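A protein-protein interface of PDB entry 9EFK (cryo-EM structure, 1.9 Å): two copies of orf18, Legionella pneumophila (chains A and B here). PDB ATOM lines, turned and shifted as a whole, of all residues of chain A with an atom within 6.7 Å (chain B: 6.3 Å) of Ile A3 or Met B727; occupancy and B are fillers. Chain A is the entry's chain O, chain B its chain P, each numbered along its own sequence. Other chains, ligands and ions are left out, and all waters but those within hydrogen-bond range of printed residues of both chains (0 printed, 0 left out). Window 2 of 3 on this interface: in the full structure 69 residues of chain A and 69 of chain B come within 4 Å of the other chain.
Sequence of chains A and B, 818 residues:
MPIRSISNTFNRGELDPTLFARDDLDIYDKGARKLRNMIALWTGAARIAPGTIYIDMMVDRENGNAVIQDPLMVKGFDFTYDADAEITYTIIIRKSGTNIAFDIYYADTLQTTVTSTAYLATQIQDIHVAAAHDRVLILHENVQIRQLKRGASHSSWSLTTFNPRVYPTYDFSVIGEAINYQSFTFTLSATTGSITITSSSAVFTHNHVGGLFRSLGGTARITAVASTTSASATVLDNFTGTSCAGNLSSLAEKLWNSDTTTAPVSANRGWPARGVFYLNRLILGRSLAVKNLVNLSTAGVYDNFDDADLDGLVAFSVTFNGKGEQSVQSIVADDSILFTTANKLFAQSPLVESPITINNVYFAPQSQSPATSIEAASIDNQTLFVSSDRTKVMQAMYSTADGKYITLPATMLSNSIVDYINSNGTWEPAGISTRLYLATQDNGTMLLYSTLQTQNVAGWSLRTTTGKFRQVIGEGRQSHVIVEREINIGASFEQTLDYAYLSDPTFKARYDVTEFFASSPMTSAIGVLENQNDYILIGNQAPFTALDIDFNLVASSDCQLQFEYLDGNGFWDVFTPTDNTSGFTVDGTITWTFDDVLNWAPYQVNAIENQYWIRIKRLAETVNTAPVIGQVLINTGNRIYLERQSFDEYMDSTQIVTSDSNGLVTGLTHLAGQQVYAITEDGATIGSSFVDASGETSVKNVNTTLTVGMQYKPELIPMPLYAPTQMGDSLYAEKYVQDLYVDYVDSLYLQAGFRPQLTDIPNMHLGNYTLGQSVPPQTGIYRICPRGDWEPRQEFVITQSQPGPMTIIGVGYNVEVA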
ATOM      1  N   PRO A   2      15.927   1.171  24.949  1.00  0.00           N
ATOM      2  CA  PRO A   2      16.564   2.353  25.537  1.00  0.00           C
ATOM      3  C   PRO A   2      16.102   3.641  24.874  1.00  0.00           C
ATOM      4  O   PRO A   2      16.536   3.945  23.767  1.00  0.00           O
ATOM      5  CB  PRO A   2      18.054   2.113  25.278  1.00  0.00           C
ATOM      6  CG  PRO A   2      18.180   0.644  25.152  1.00  0.00           C
ATOM      7  CD  PRO A   2      16.918   0.187  24.487  1.00  0.00           C
ATOM      8  N   ILE A   3      15.231   4.382  25.548  1.00  0.00           N
ATOM      9  CA  ILE A   3      14.714   5.632  25.006  1.00  0.00           C
ATOM     10  C   ILE A   3      15.692   6.752  25.325  1.00  0.00           C
ATOM     11  O   ILE A   3      16.151   6.890  26.463  1.00  0.00           O
ATOM     12  CB  ILE A   3      13.315   5.936  25.564  1.00  0.00           C
ATOM     13  CG1 ILE A   3      12.241   5.199  24.762  1.00  0.00           C
ATOM     14  CG2 ILE A   3      13.037   7.426  25.533  1.00  0.00           C
ATOM     15  CD1 ILE A   3      12.143   3.727  25.057  1.00  0.00           C
ATOM     16  N   ARG A   4      16.024   7.546  24.314  1.00  0.00           N
ATOM     17  CA  ARG A   4      16.895   8.698  24.467  1.00  0.00           C
ATOM     18  C   ARG A   4      16.163   9.943  23.996  1.00  0.00           C
ATOM     19  O   ARG A   4      15.394   9.893  23.034  1.00  0.00           O
ATOM     20  CB  ARG A   4      18.193   8.517  23.678  1.00  0.00           C
ATOM     21  CG  ARG A   4      18.895   7.207  23.962  1.00  0.00           C
ATOM     22  CD  ARG A   4      20.396   7.333  23.810  1.00  0.00           C
ATOM     23  NE  ARG A   4      20.974   8.217  24.815  1.00  0.00           N
ATOM     24  CZ  ARG A   4      21.436   9.434  24.568  1.00  0.00           C
ATOM     25  NH1 ARG A   4      21.428   9.942  23.349  1.00  0.00           N
ATOM     26  NH2 ARG A   4      21.922  10.158  25.571  1.00  0.00           N
ATOM     27  N   SER A   5      16.393  11.055  24.682  1.00  0.00           N
ATOM     28  CA  SER A   5      15.804  12.335  24.321  1.00  0.00           C
ATOM     29  C   SER A   5      16.864  13.187  23.644  1.00  0.00           C
ATOM     30  O   SER A   5      17.902  13.480  24.242  1.00  0.00           O
ATOM     31  CB  SER A   5      15.248  13.050  25.549  1.00  0.00           C
ATOM     32  OG  SER A   5      14.222  12.289  26.149  1.00  0.00           O
ATOM     33  N   ILE A   6      16.600  13.584  22.403  1.00  0.00           N
ATOM     34  CA  ILE A   6      17.528  14.379  21.617  1.00  0.00           C
ATOM     35  C   ILE A   6      16.768  15.555  21.022  1.00  0.00           C
ATOM     36  O   ILE A   6      15.540  15.552  20.941  1.00  0.00           O
ATOM     37  CB  ILE A   6      18.205  13.552  20.510  1.00  0.00           C
ATOM     38  CG1 ILE A   6      17.153  12.915  19.608  1.00  0.00           C
ATOM     39  CG2 ILE A   6      19.081  12.475  21.115  1.00  0.00           C
ATOM     40  CD1 ILE A   6      17.732  12.090  18.494  1.00  0.00           C
ATOM     41  N   GLN A 738       9.314   7.538  18.940  1.00  0.00           N
ATOM     42  CA  GLN A 738       8.042   7.423  19.639  1.00  0.00           C
ATOM     43  C   GLN A 738       7.325   8.763  19.711  1.00  0.00           C
ATOM     44  O   GLN A 738       6.111   8.834  19.501  1.00  0.00           O
ATOM     45  CB  GLN A 738       8.264   6.852  21.038  1.00  0.00           C
ATOM     46  CG  GLN A 738       8.793   5.440  21.037  1.00  0.00           C
ATOM     47  CD  GLN A 738       8.841   4.838  22.418  1.00  0.00           C
ATOM     48  OE1 GLN A 738       9.193   5.506  23.381  1.00  0.00           O
ATOM     49  NE2 GLN A 738       8.481   3.571  22.523  1.00  0.00           N
ATOM     50  N   TYR A 813      12.940  14.710  20.064  1.00  0.00           N
ATOM     51  CA  TYR A 813      12.508  13.341  19.827  1.00  0.00           C
ATOM     52  C   TYR A 813      12.661  12.515  21.093  1.00  0.00           C
ATOM     53  O   TYR A 813      13.518  12.789  21.935  1.00  0.00           O
ATOM     54  CB  TYR A 813      13.314  12.643  18.729  1.00  0.00           C
ATOM     55  CG  TYR A 813      13.588  13.437  17.481  1.00  0.00           C
ATOM     56  CD1 TYR A 813      14.689  14.266  17.397  1.00  0.00           C
ATOM     57  CD2 TYR A 813      12.777  13.315  16.370  1.00  0.00           C
ATOM     58  CE1 TYR A 813      14.954  14.975  16.258  1.00  0.00           C
ATOM     59  CE2 TYR A 813      13.039  14.017  15.222  1.00  0.00           C
ATOM     60  CZ  TYR A 813      14.127  14.848  15.173  1.00  0.00           C
ATOM     61  OH  TYR A 813      14.394  15.554  14.031  1.00  0.00           O
ATOM     62  N   ASN A 814      11.832  11.488  21.205  1.00  0.00           N
ATOM     63  CA  ASN A 814      12.067  10.357  22.095  1.00  0.00           C
ATOM     64  C   ASN A 814      12.301   9.153  21.196  1.00  0.00           C
ATOM     65  O   ASN A 814      11.363   8.653  20.571  1.00  0.00           O
ATOM     66  CB  ASN A 814      10.892  10.121  23.038  1.00  0.00           C
ATOM     67  CG  ASN A 814      10.772  11.185  24.098  1.00  0.00           C
ATOM     68  OD1 ASN A 814      11.759  11.791  24.496  1.00  0.00           O
ATOM     69  ND2 ASN A 814       9.557  11.417  24.565  1.00  0.00           N
ATOM     70  N   VAL A 815      13.543   8.695  21.116  1.00  0.00           N
ATOM     71  CA  VAL A 815      13.945   7.682  20.150  1.00  0.00           C
ATOM     72  C   VAL A 815      14.230   6.378  20.879  1.00  0.00           C
ATOM     73  O   VAL A 815      14.998   6.352  21.845  1.00  0.00           O
ATOM     74  CB  VAL A 815      15.176   8.126  19.346  1.00  0.00           C
ATOM     75  CG1 VAL A 815      15.352   7.246  18.130  1.00  0.00           C
ATOM     76  CG2 VAL A 815      15.042   9.559  18.938  1.00  0.00           C
ATOM     77  N   GLU A 816      13.618   5.298  20.409  1.00  0.00           N
ATOM     78  CA  GLU A 816      13.998   3.953  20.817  1.00  0.00           C
ATOM     79  C   GLU A 816      15.161   3.509  19.941  1.00  0.00           C
ATOM     80  O   GLU A 816      14.986   3.253  18.747  1.00  0.00           O
ATOM     81  CB  GLU A 816      12.804   3.009  20.699  1.00  0.00           C
ATOM     82  CG  GLU A 816      13.146   1.528  20.653  1.00  0.00           C
ATOM     83  CD  GLU A 816      13.698   1.001  21.960  1.00  0.00           C
ATOM     84  OE1 GLU A 816      13.435   1.614  23.013  1.00  0.00           O
ATOM     85  OE2 GLU A 816      14.399  -0.032  21.934  1.00  0.00           O
ATOM     86  N   VAL A 817      16.355   3.447  20.516  1.00  0.00           N
ATOM     87  CA  VAL A 817      17.561   3.091  19.780  1.00  0.00           C
ATOM     88  C   VAL A 817      17.788   1.599  19.980  1.00  0.00           C
ATOM     89  O   VAL A 817      18.224   1.158  21.046  1.00  0.00           O
ATOM     90  CB  VAL A 817      18.770   3.912  20.228  1.00  0.00           C
ATOM     91  CG1 VAL A 817      20.000   3.473  19.470  1.00  0.00           C
ATOM     92  CG2 VAL A 817      18.516   5.382  19.996  1.00  0.00           C
ATOM     93  N   THR B 725      19.275  14.580  32.195  1.00  0.00           N
ATOM     94  CA  THR B 725      19.454  13.297  32.862  1.00  0.00           C
ATOM     95  C   THR B 725      20.362  12.416  32.009  1.00  0.00           C
ATOM     96  O   THR B 725      20.955  12.864  31.024  1.00  0.00           O
ATOM     97  CB  THR B 725      18.106  12.619  33.119  1.00  0.00           C
ATOM     98  OG1 THR B 725      17.494  12.274  31.871  1.00  0.00           O
ATOM     99  CG2 THR B 725      17.178  13.539  33.890  1.00  0.00           C
ATOM    100  N   GLN B 726      20.483  11.149  32.406  1.00  0.00           N
ATOM    101  CA  GLN B 726      21.256  10.206  31.606  1.00  0.00           C
ATOM    102  C   GLN B 726      20.546   9.859  30.303  1.00  0.00           C
ATOM    103  O   GLN B 726      21.206   9.606  29.290  1.00  0.00           O
ATOM    104  CB  GLN B 726      21.546   8.939  32.412  1.00  0.00           C
ATOM    105  CG  GLN B 726      20.351   8.374  33.165  1.00  0.00           C
ATOM    106  CD  GLN B 726      20.198   8.969  34.553  1.00  0.00           C
ATOM    107  OE1 GLN B 726      21.046   9.737  35.008  1.00  0.00           O
ATOM    108  NE2 GLN B 726      19.113   8.616  35.234  1.00  0.00           N
ATOM    109  N   MET B 727      19.210   9.852  30.306  1.00  0.00           N
ATOM    110  CA  MET B 727      18.465   9.543  29.090  1.00  0.00           C
ATOM    111  C   MET B 727      18.737  10.567  27.997  1.00  0.00           C
ATOM    112  O   MET B 727      18.885  10.209  26.824  1.00  0.00           O
ATOM    113  CB  MET B 727      16.969   9.483  29.389  1.00  0.00           C
ATOM    114  CG  MET B 727      16.565   8.410  30.378  1.00  0.00           C
ATOM    115  SD  MET B 727      14.798   8.449  30.726  1.00  0.00           S
ATOM    116  CE  MET B 727      14.123   8.384  29.069  1.00  0.00           C
ATOM    117  N   GLY B 728      18.801  11.842  28.357  1.00  0.00           N
ATOM    118  CA  GLY B 728      19.027  12.880  27.376  1.00  0.00           C
ATOM    119  C   GLY B 728      18.794  14.247  27.986  1.00  0.00           C
ATOM    120  O   GLY B 728      18.732  14.400  29.206  1.00  0.00           O
ATOM    121  N   ASP B 729      18.660  15.238  27.102  1.00  0.00           N
ATOM    122  CA  ASP B 729      18.500  16.614  27.559  1.00  0.00           C
ATOM    123  C   ASP B 729      17.198  16.812  28.321  1.00  0.00           C
ATOM    124  O   ASP B 729      17.122  17.681  29.195  1.00  0.00           O
ATOM    125  CB  ASP B 729      18.578  17.578  26.374  1.00  0.00           C
ATOM    126  CG  ASP B 729      17.639  17.201  25.243  1.00  0.00           C
ATOM    127  OD1 ASP B 729      16.409  17.261  25.430  1.00  0.00           O
ATOM    128  OD2 ASP B 729      18.134  16.857  24.152  1.00  0.00           O
ATOM    129  N   SER B 730      16.171  16.022  28.008  1.00  0.00           N
ATOM    130  CA  SER B 730      14.867  16.115  28.670  1.00  0.00           C
ATOM    131  C   SER B 730      14.298  17.529  28.593  1.00  0.00           C
ATOM    132  O   SER B 730      13.621  17.994  29.508  1.00  0.00           O
ATOM    133  CB  SER B 730      14.946  15.640  30.121  1.00  0.00           C
ATOM    134  OG  SER B 730      15.157  14.241  30.183  1.00  0.00           O
ATOM    135  N   ALA B 818       9.942  13.317  34.782  1.00  0.00           N
ATOM    136  CA  ALA B 818       9.334  12.091  34.289  1.00  0.00           C
ATOM    137  C   ALA B 818       9.802  11.799  32.872  1.00  0.00           C
ATOM    138  O   ALA B 818       9.402  12.476  31.928  1.00  0.00           O
ATOM    139  CB  ALA B 818       7.819  12.191  34.340  1.00  0.00           C
ATOM    140  OXT ALA B 818      10.585  10.880  32.640  1.00  0.00           O
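N of Asp B729 lies within hydrogen-bond range of O of Ser A5, at 3.4 Å. The backbone carbonyl oxygen of Met B727 is in hydrogen-bond range of the backbone NH of Ser A5, 3.4 Å away. NH2 of Arg A4 sits at hydrogen-bond distance from O of Met B727 (3.3 Å).
Hydrophobic or aromatic side chains of chain A that line the printed part of chain B: Ile A3. Hydrophobic or aromatic side chains of chain B within 4 Å of the printed part of chain A: Met B727. Among the printed residues, no Asp or Glu carboxylate lies within 4 Å of a Lys or Arg side-chain nitrogen of the other chain.
No position is printed for both chains. Of the 8 pairs that touch across the chains among the printed residues, none has its exchanged pair printed and touching as well.
O of Ile A6 sits at hydrogen-bond distance from N of Tyr A813, 2.9 Å away. O of Arg A4 is in hydrogen-bond range of N of Val A815. The side-chain hydroxyl (OG1) of Thr B725 is in hydrogen-bond range of the side-chain hydroxyl (OG) of Ser B730, 3.5 Å away. The side-chain amide oxygen (OD1) of Asn A814 lies within hydrogen-bond range of the side-chain hydroxyl (OG) of Ser A5. The side-chain hydroxyl (OG1) of Thr B725 lies close to the backbone NH (N) of Met B727 (3.4 Å).
Ile A3 touches just one residue of chain B: Met B727. Of the printed residues of chain B, Ile A6 touches Asp B729 (3.6 Å). Of the printed residues of chain A, Ser B730 touches Ser A5 (3.97 Å). Of the printed residues of chain A, Asp B729 touches Ser A5 (3.4 Å) and Ile A6 (3.6 Å). Of the printed residues of chain B, Arg A4 touches Gln B726 and Met B727. Glu A816 touches none of the printed residues of chain B. Thr B725 touches none of the printed residues of chain A.
Among the printed residues, pairs that only touch across the chains: Ser A5 with Gly B728 (3.4 Å), Ile A6 with Asp B729 (3.6 Å), Ile A3 with Met B727 (3.6 Å), Arg A4 with Gln B726 (3.8 Å) and Ser A5 with Ser B730 (3.97 Å).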
